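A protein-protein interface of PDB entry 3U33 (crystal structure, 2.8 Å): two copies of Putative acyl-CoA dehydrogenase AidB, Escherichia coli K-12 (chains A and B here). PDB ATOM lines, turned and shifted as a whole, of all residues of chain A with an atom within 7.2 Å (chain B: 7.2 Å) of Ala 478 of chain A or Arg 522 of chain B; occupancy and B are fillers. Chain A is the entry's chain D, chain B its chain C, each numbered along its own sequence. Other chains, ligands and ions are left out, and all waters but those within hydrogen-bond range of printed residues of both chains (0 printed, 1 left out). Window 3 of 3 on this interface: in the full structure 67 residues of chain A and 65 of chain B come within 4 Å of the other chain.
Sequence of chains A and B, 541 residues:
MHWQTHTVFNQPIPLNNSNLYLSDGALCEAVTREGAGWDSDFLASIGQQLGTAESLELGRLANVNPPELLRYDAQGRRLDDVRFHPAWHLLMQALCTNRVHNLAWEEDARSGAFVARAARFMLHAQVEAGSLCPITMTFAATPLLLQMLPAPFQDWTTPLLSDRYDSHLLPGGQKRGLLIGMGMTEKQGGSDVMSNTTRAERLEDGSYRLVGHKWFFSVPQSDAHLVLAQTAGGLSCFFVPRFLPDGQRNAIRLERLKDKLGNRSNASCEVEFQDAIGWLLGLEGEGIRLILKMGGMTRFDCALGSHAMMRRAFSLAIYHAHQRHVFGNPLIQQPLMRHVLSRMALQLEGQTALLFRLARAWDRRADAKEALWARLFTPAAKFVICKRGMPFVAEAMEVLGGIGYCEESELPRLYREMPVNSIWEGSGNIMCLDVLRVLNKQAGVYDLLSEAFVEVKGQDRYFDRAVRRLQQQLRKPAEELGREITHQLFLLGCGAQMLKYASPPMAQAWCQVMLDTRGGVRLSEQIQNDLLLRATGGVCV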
ATOM      1  N   LEU A 436      27.257  23.877  29.699  1.00  0.00           N
ATOM      2  CA  LEU A 436      28.358  22.965  29.971  1.00  0.00           C
ATOM      3  C   LEU A 436      29.630  23.734  30.307  1.00  0.00           C
ATOM      4  O   LEU A 436      30.359  23.363  31.224  1.00  0.00           O
ATOM      5  CB  LEU A 436      28.606  22.028  28.793  1.00  0.00           C
ATOM      6  CG  LEU A 436      27.554  20.946  28.541  1.00  0.00           C
ATOM      7  CD1 LEU A 436      28.013  20.002  27.426  1.00  0.00           C
ATOM      8  CD2 LEU A 436      27.230  20.162  29.811  1.00  0.00           C
ATOM      9  N   GLN A 473      25.451  12.089  36.177  1.00  0.00           N
ATOM     10  CA  GLN A 473      25.627  12.506  34.793  1.00  0.00           C
ATOM     11  C   GLN A 473      26.693  13.585  34.643  1.00  0.00           C
ATOM     12  O   GLN A 473      27.186  13.826  33.543  1.00  0.00           O
ATOM     13  CB  GLN A 473      24.307  13.030  34.232  1.00  0.00           C
ATOM     14  CG  GLN A 473      24.268  13.094  32.721  1.00  0.00           C
ATOM     15  CD  GLN A 473      23.906  11.760  32.109  1.00  0.00           C
ATOM     16  OE1 GLN A 473      22.751  11.522  31.763  1.00  0.00           O
ATOM     17  NE2 GLN A 473      24.891  10.878  31.980  1.00  0.00           N
ATOM     18  N   LEU A 474      27.032  14.246  35.746  1.00  0.00           N
ATOM     19  CA  LEU A 474      28.060  15.282  35.732  1.00  0.00           C
ATOM     20  C   LEU A 474      29.428  14.664  35.995  1.00  0.00           C
ATOM     21  O   LEU A 474      30.451  15.358  35.978  1.00  0.00           O
ATOM     22  CB  LEU A 474      27.755  16.367  36.766  1.00  0.00           C
ATOM     23  CG  LEU A 474      26.403  17.065  36.610  1.00  0.00           C
ATOM     24  CD1 LEU A 474      26.210  18.143  37.665  1.00  0.00           C
ATOM     25  CD2 LEU A 474      26.273  17.656  35.221  1.00  0.00           C
ATOM     26  N   ARG A 475      29.434  13.356  36.245  1.00  0.00           N
ATOM     27  CA  ARG A 475      30.674  12.597  36.359  1.00  0.00           C
ATOM     28  C   ARG A 475      31.509  12.785  35.092  1.00  0.00           C
ATOM     29  O   ARG A 475      32.597  13.362  35.141  1.00  0.00           O
ATOM     30  CB  ARG A 475      30.385  11.111  36.601  1.00  0.00           C
ATOM     31  N   LYS A 476      30.985  12.311  33.960  1.00  0.00           N
ATOM     32  CA  LYS A 476      31.629  12.508  32.660  1.00  0.00           C
ATOM     33  C   LYS A 476      30.829  13.471  31.780  1.00  0.00           C
ATOM     34  O   LYS A 476      30.065  13.034  30.920  1.00  0.00           O
ATOM     35  CB  LYS A 476      31.804  11.169  31.940  1.00  0.00           C
ATOM     36  N   PRO A 477      31.012  14.789  31.986  1.00  0.00           N
ATOM     37  CA  PRO A 477      30.224  15.818  31.292  1.00  0.00           C
ATOM     38  C   PRO A 477      30.475  15.823  29.787  1.00  0.00           C
ATOM     39  O   PRO A 477      31.220  16.677  29.301  1.00  0.00           O
ATOM     40  CB  PRO A 477      30.733  17.129  31.906  1.00  0.00           C
ATOM     41  CG  PRO A 477      31.446  16.731  33.166  1.00  0.00           C
ATOM     42  CD  PRO A 477      32.020  15.383  32.881  1.00  0.00           C
ATOM     43  N   ALA A 478      29.851  14.889  29.067  1.00  0.00           N
ATOM     44  CA  ALA A 478      30.071  14.732  27.629  1.00  0.00           C
ATOM     45  C   ALA A 478      29.286  15.748  26.808  1.00  0.00           C
ATOM     46  O   ALA A 478      28.117  16.011  27.083  1.00  0.00           O
ATOM     47  CB  ALA A 478      29.720  13.324  27.193  1.00  0.00           C
ATOM     48  N   GLU A 479      29.934  16.301  25.788  1.00  0.00           N
ATOM     49  CA  GLU A 479      29.341  17.355  24.973  1.00  0.00           C
ATOM     50  C   GLU A 479      28.027  16.946  24.274  1.00  0.00           C
ATOM     51  O   GLU A 479      27.080  17.726  24.248  1.00  0.00           O
ATOM     52  CB  GLU A 479      30.370  17.861  23.959  1.00  0.00           C
ATOM     53  CG  GLU A 479      29.971  19.131  23.228  1.00  0.00           C
ATOM     54  CD  GLU A 479      31.003  19.557  22.198  1.00  0.00           C
ATOM     55  OE1 GLU A 479      32.089  18.944  22.161  1.00  0.00           O
ATOM     56  OE2 GLU A 479      30.732  20.499  21.424  1.00  0.00           O
ATOM     57  N   GLU A 480      27.973  15.736  23.712  1.00  0.00           N
ATOM     58  CA  GLU A 480      26.763  15.231  23.055  1.00  0.00           C
ATOM     59  C   GLU A 480      25.576  15.103  24.014  1.00  0.00           C
ATOM     60  O   GLU A 480      24.428  14.992  23.585  1.00  0.00           O
ATOM     61  CB  GLU A 480      27.043  13.888  22.381  1.00  0.00           C
ATOM     62  CG  GLU A 480      28.155  13.095  23.042  1.00  0.00           C
ATOM     63  CD  GLU A 480      28.570  11.884  22.228  1.00  0.00           C
ATOM     64  OE1 GLU A 480      27.689  11.245  21.605  1.00  0.00           O
ATOM     65  OE2 GLU A 480      29.783  11.580  22.207  1.00  0.00           O
ATOM     66  N   LEU A 481      25.854  15.125  25.311  1.00  0.00           N
ATOM     67  CA  LEU A 481      24.798  15.046  26.310  1.00  0.00           C
ATOM     68  C   LEU A 481      24.413  16.430  26.817  1.00  0.00           C
ATOM     69  O   LEU A 481      23.701  16.560  27.813  1.00  0.00           O
ATOM     70  CB  LEU A 481      25.233  14.165  27.479  1.00  0.00           C
ATOM     71  CG  LEU A 481      25.482  12.692  27.169  1.00  0.00           C
ATOM     72  CD1 LEU A 481      25.967  11.962  28.416  1.00  0.00           C
ATOM     73  CD2 LEU A 481      24.225  12.044  26.619  1.00  0.00           C
ATOM     74  N   GLY A 482      24.888  17.461  26.128  1.00  0.00           N
ATOM     75  CA  GLY A 482      24.630  18.834  26.523  1.00  0.00           C
ATOM     76  C   GLY A 482      23.161  19.171  26.689  1.00  0.00           C
ATOM     77  O   GLY A 482      22.795  19.980  27.532  1.00  0.00           O
ATOM     78  N   ARG A 483      22.307  18.553  25.885  1.00  0.00           N
ATOM     79  CA  ARG A 483      20.879  18.806  26.001  1.00  0.00           C
ATOM     80  C   ARG A 483      20.265  18.041  27.163  1.00  0.00           C
ATOM     81  O   ARG A 483      19.506  18.604  27.948  1.00  0.00           O
ATOM     82  CB  ARG A 483      20.156  18.449  24.710  1.00  0.00           C
ATOM     83  CG  ARG A 483      20.399  19.411  23.580  1.00  0.00           C
ATOM     84  CD  ARG A 483      19.414  19.131  22.476  1.00  0.00           C
ATOM     85  NE  ARG A 483      19.507  20.092  21.386  1.00  0.00           N
ATOM     86  CZ  ARG A 483      18.558  20.260  20.474  1.00  0.00           C
ATOM     87  NH1 ARG A 483      17.447  19.534  20.536  1.00  0.00           N
ATOM     88  NH2 ARG A 483      18.715  21.153  19.509  1.00  0.00           N
ATOM     89  N   GLU A 484      20.583  16.757  27.268  1.00  0.00           N
ATOM     90  CA  GLU A 484      20.077  15.951  28.368  1.00  0.00           C
ATOM     91  C   GLU A 484      20.445  16.613  29.695  1.00  0.00           C
ATOM     92  O   GLU A 484      19.631  16.688  30.614  1.00  0.00           O
ATOM     93  CB  GLU A 484      20.655  14.536  28.308  1.00  0.00           C
ATOM     94  CG  GLU A 484      20.680  13.930  26.920  1.00  0.00           C
ATOM     95  CD  GLU A 484      19.295  13.656  26.371  1.00  0.00           C
ATOM     96  OE1 GLU A 484      18.500  12.990  27.066  1.00  0.00           O
ATOM     97  OE2 GLU A 484      19.003  14.103  25.241  1.00  0.00           O
ATOM     98  N   ILE A 485      21.678  17.102  29.779  1.00  0.00           N
ATOM     99  CA  ILE A 485      22.189  17.716  31.000  1.00  0.00           C
ATOM    100  C   ILE A 485      21.504  19.041  31.303  1.00  0.00           C
ATOM    101  O   ILE A 485      21.039  19.268  32.415  1.00  0.00           O
ATOM    102  CB  ILE A 485      23.715  17.921  30.921  1.00  0.00           C
ATOM    103  CG1 ILE A 485      24.437  16.573  31.088  1.00  0.00           C
ATOM    104  CG2 ILE A 485      24.175  18.919  31.982  1.00  0.00           C
ATOM    105  CD1 ILE A 485      25.914  16.596  30.737  1.00  0.00           C
ATOM    106  N   PRO B 335      29.598  17.292  17.736  1.00  0.00           N
ATOM    107  CA  PRO B 335      29.072  16.261  18.640  1.00  0.00           C
ATOM    108  C   PRO B 335      27.595  16.438  19.006  1.00  0.00           C
ATOM    109  O   PRO B 335      26.807  15.522  18.788  1.00  0.00           O
ATOM    110  CB  PRO B 335      29.953  16.415  19.875  1.00  0.00           C
ATOM    111  CG  PRO B 335      31.248  16.892  19.325  1.00  0.00           C
ATOM    112  CD  PRO B 335      30.933  17.757  18.147  1.00  0.00           C
ATOM    113  N   LEU B 336      27.227  17.592  19.552  1.00  0.00           N
ATOM    114  CA  LEU B 336      25.847  17.819  19.973  1.00  0.00           C
ATOM    115  C   LEU B 336      24.864  17.778  18.802  1.00  0.00           C
ATOM    116  O   LEU B 336      23.790  17.199  18.923  1.00  0.00           O
ATOM    117  CB  LEU B 336      25.714  19.140  20.737  1.00  0.00           C
ATOM    118  CG  LEU B 336      24.345  19.397  21.374  1.00  0.00           C
ATOM    119  CD1 LEU B 336      23.878  18.187  22.170  1.00  0.00           C
ATOM    120  CD2 LEU B 336      24.375  20.637  22.253  1.00  0.00           C
ATOM    121  N   HIS B 339      24.405  14.328  17.413  1.00  0.00           N
ATOM    122  CA  HIS B 339      23.586  13.579  18.367  1.00  0.00           C
ATOM    123  C   HIS B 339      22.093  13.824  18.119  1.00  0.00           C
ATOM    124  O   HIS B 339      21.294  12.887  18.045  1.00  0.00           O
ATOM    125  CB  HIS B 339      23.971  13.971  19.802  1.00  0.00           C
ATOM    126  CG  HIS B 339      23.115  13.348  20.862  1.00  0.00           C
ATOM    127  ND1 HIS B 339      23.255  12.036  21.260  1.00  0.00           N
ATOM    128  CD2 HIS B 339      22.116  13.864  21.618  1.00  0.00           C
ATOM    129  CE1 HIS B 339      22.375  11.768  22.209  1.00  0.00           C
ATOM    130  NE2 HIS B 339      21.673  12.861  22.445  1.00  0.00           N
ATOM    131  N   ARG B 343      19.231  11.087  16.609  1.00  0.00           N
ATOM    132  CA  ARG B 343      17.974  10.780  17.278  1.00  0.00           C
ATOM    133  C   ARG B 343      16.794  11.048  16.346  1.00  0.00           C
ATOM    134  O   ARG B 343      15.806  10.311  16.356  1.00  0.00           O
ATOM    135  CB  ARG B 343      17.849  11.569  18.588  1.00  0.00           C
ATOM    136  CG  ARG B 343      18.833  11.109  19.648  1.00  0.00           C
ATOM    137  CD  ARG B 343      18.848  12.021  20.857  1.00  0.00           C
ATOM    138  NE  ARG B 343      17.726  11.788  21.755  1.00  0.00           N
ATOM    139  CZ  ARG B 343      17.793  11.200  22.946  1.00  0.00           C
ATOM    140  NH1 ARG B 343      16.681  11.061  23.648  1.00  0.00           N
ATOM    141  NH2 ARG B 343      18.943  10.758  23.443  1.00  0.00           N
ATOM    142  N   GLN B 512      16.813   1.564  23.200  1.00  0.00           N
ATOM    143  CA  GLN B 512      17.467   2.331  24.251  1.00  0.00           C
ATOM    144  C   GLN B 512      16.962   3.769  24.248  1.00  0.00           C
ATOM    145  O   GLN B 512      16.437   4.256  25.248  1.00  0.00           O
ATOM    146  CB  GLN B 512      18.990   2.297  24.085  1.00  0.00           C
ATOM    147  CG  GLN B 512      19.754   2.502  25.383  1.00  0.00           C
ATOM    148  CD  GLN B 512      21.214   2.116  25.270  1.00  0.00           C
ATOM    149  OE1 GLN B 512      21.715   1.843  24.175  1.00  0.00           O
ATOM    150  NE2 GLN B 512      21.908   2.088  26.406  1.00  0.00           N
ATOM    151  N   VAL B 513      17.102   4.441  23.114  1.00  0.00           N
ATOM    152  CA  VAL B 513      16.717   5.841  23.019  1.00  0.00           C
ATOM    153  C   VAL B 513      15.239   6.110  23.330  1.00  0.00           C
ATOM    154  O   VAL B 513      14.912   7.112  23.973  1.00  0.00           O
ATOM    155  CB  VAL B 513      17.063   6.421  21.640  1.00  0.00           C
ATOM    156  CG1 VAL B 513      16.430   7.793  21.466  1.00  0.00           C
ATOM    157  CG2 VAL B 513      18.564   6.496  21.466  1.00  0.00           C
ATOM    158  N   GLY B 519      17.531   7.879  30.625  1.00  0.00           N
ATOM    159  CA  GLY B 519      18.057   8.985  29.848  1.00  0.00           C
ATOM    160  C   GLY B 519      19.572   8.975  29.833  1.00  0.00           C
ATOM    161  O   GLY B 519      20.199   8.043  30.342  1.00  0.00           O
ATOM    162  N   GLY B 520      20.163  10.015  29.252  1.00  0.00           N
ATOM    163  CA  GLY B 520      21.609  10.102  29.129  1.00  0.00           C
ATOM    164  C   GLY B 520      22.146   9.085  28.143  1.00  0.00           C
ATOM    165  O   GLY B 520      23.244   8.556  28.315  1.00  0.00           O
ATOM    166  N   VAL B 521      21.363   8.829  27.098  1.00  0.00           N
ATOM    167  CA  VAL B 521      21.657   7.775  26.133  1.00  0.00           C
ATOM    168  C   VAL B 521      22.604   8.238  25.039  1.00  0.00           C
ATOM    169  O   VAL B 521      22.211   8.968  24.133  1.00  0.00           O
ATOM    170  CB  VAL B 521      20.370   7.272  25.445  1.00  0.00           C
ATOM    171  CG1 VAL B 521      20.616   5.919  24.789  1.00  0.00           C
ATOM    172  CG2 VAL B 521      19.215   7.199  26.443  1.00  0.00           C
ATOM    173  N   ARG B 522      23.852   7.805  25.118  1.00  0.00           N
ATOM    174  CA  ARG B 522      24.809   8.089  24.061  1.00  0.00           C
ATOM    175  C   ARG B 522      24.738   6.992  23.010  1.00  0.00           C
ATOM    176  O   ARG B 522      24.441   5.841  23.328  1.00  0.00           O
ATOM    177  CB  ARG B 522      26.225   8.174  24.623  1.00  0.00           C
ATOM    178  CG  ARG B 522      26.454   9.344  25.557  1.00  0.00           C
ATOM    179  CD  ARG B 522      27.832   9.291  26.197  1.00  0.00           C
ATOM    180  NE  ARG B 522      28.870   9.912  25.377  1.00  0.00           N
ATOM    181  CZ  ARG B 522      30.139  10.037  25.760  1.00  0.00           C
ATOM    182  NH1 ARG B 522      30.523   9.581  26.948  1.00  0.00           N
ATOM    183  NH2 ARG B 522      31.026  10.617  24.962  1.00  0.00           N
ATOM    184  N   LEU B 523      25.004   7.350  21.757  1.00  0.00           N
ATOM    185  CA  LEU B 523      24.996   6.376  20.666  1.00  0.00           C
ATOM    186  C   LEU B 523      26.400   6.152  20.128  1.00  0.00           C
ATOM    187  O   LEU B 523      27.183   7.098  20.008  1.00  0.00           O
ATOM    188  CB  LEU B 523      24.075   6.826  19.533  1.00  0.00           C
ATOM    189  CG  LEU B 523      22.573   6.786  19.813  1.00  0.00           C
ATOM    190  CD1 LEU B 523      21.805   7.370  18.644  1.00  0.00           C
ATOM    191  CD2 LEU B 523      22.116   5.370  20.094  1.00  0.00           C
ATOM    192  N   SER B 524      26.715   4.901  19.806  1.00  0.00           N
ATOM    193  CA  SER B 524      28.034   4.563  19.285  1.00  0.00           C
ATOM    194  C   SER B 524      28.344   5.379  18.038  1.00  0.00           C
ATOM    195  O   SER B 524      27.445   5.738  17.277  1.00  0.00           O
ATOM    196  CB  SER B 524      28.141   3.067  18.976  1.00  0.00           C
ATOM    197  OG  SER B 524      27.287   2.694  17.911  1.00  0.00           O
ATOM    198  N   ILE B 527      26.870   3.547  14.949  1.00  0.00           N
ATOM    199  CA  ILE B 527      25.423   3.535  14.745  1.00  0.00           C
ATOM    200  C   ILE B 527      24.926   4.888  14.248  1.00  0.00           C
ATOM    201  O   ILE B 527      23.989   4.962  13.451  1.00  0.00           O
ATOM    202  CB  ILE B 527      24.652   3.127  16.018  1.00  0.00           C
ATOM    203  CG1 ILE B 527      23.231   2.668  15.665  1.00  0.00           C
ATOM    204  CG2 ILE B 527      24.607   4.271  17.005  1.00  0.00           C
ATOM    205  CD1 ILE B 527      23.181   1.454  14.753  1.00  0.00           C
ATOM    206  N   GLN B 528      25.564   5.960  14.704  1.00  0.00           N
ATOM    207  CA  GLN B 528      25.225   7.287  14.214  1.00  0.00           C
ATOM    208  C   GLN B 528      25.578   7.432  12.734  1.00  0.00           C
ATOM    209  O   GLN B 528      24.772   7.925  11.942  1.00  0.00           O
ATOM    210  CB  GLN B 528      25.901   8.368  15.059  1.00  0.00           C
ATOM    211  CG  GLN B 528      25.304   8.518  16.450  1.00  0.00           C
ATOM    212  CD  GLN B 528      25.771   9.779  17.148  1.00  0.00           C
ATOM    213  OE1 GLN B 528      26.738  10.415  16.721  1.00  0.00           O
ATOM    214  NE2 GLN B 528      25.082  10.150  18.230  1.00  0.00           N
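Hydrophobic or aromatic side chains of chain B that line the printed part of chain A: Pro 335, Leu 336 and His 339.
Among the printed residues, 12 pairs touch across the chains.
Among the printed residues, Asp or Glu carboxylates within 4 Å of a Lys or Arg side-chain nitrogen of the other chain: Glu 480 of chain A with Arg 522 of chain B (3.2 Å) and Glu 484 of chain A with Arg 343 of chain B (3.8 Å).
The side-chain carboxylate of Glu 480 of chain A lies within salt-bridge range of the guanidinium group of Arg 522 of chain B (3.2 Å).
The side-chain carboxylate (OE2) of Glu 484 of chain A lies within salt-bridge range of the guanidinium group (NH2) of Arg 343 of chain B.
No position is printed for both chains.
Of the 12 pairs that touch across the chains among the printed residues, none has its exchanged pair printed and touching as well.
OE1 of Gln 473 of chain A touches CA of Gly 520 of chain B (3.2 Å).
Arg 522 of chain B touches Ala 478 of chain A.
Pro 335 of chain B touches Glu 479 of chain A.
O of Glu 479 of chain A touches CD1 of Leu 336 of chain B, 3.8 Å away.
CB of Glu 480 of chain A touches O of Pro 335 of chain B, at 3.95 Å.
Leu 336 of chain B touches Glu 480 of chain A.
CD2 of His 339 of chain B touches O of Glu 480 of chain A, 3.2 Å away.
Leu 481 of chain A touches Gly 520 of chain B (CD2 to C, 3.9 Å).
Arg 522 of chain B touches Leu 481 of chain A.
Arg 483 of chain A touches Leu 336 of chain B.
Arg 475 of chain A touches none of the printed residues of chain B.
Ala 478 of chain A touches just one residue of chain B: Arg 522 (3.6 Å).
Of the printed residues of chain B, Leu 481 of chain A touches Gly 520 (3.9 Å) and Arg 522 (3.7 Å).
Of the printed residues of chain B, Arg 483 of chain A touches Leu 336.
Printed residues of chain B within 4 Å of Glu 484 of chain A: Arg 343 (3.8 Å).
Printed residues of chain A within 4 Å of Arg 522 of chain B: Ala 478 (3.6 Å), Glu 480 (3.2 Å) and Leu 481 (3.7 Å).
The nearest residue of chain B that does not touch Ala 478 of chain A is Leu 336 of chain B (6.8 Å).
The nearest residue of chain A that does not touch Arg 522 of chain B is Lys 476 of chain A (5.3 Å).
The nearest printed residue of chain A that does not touch Arg 343 of chain B is Leu 481 of chain A (6.3 Å).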
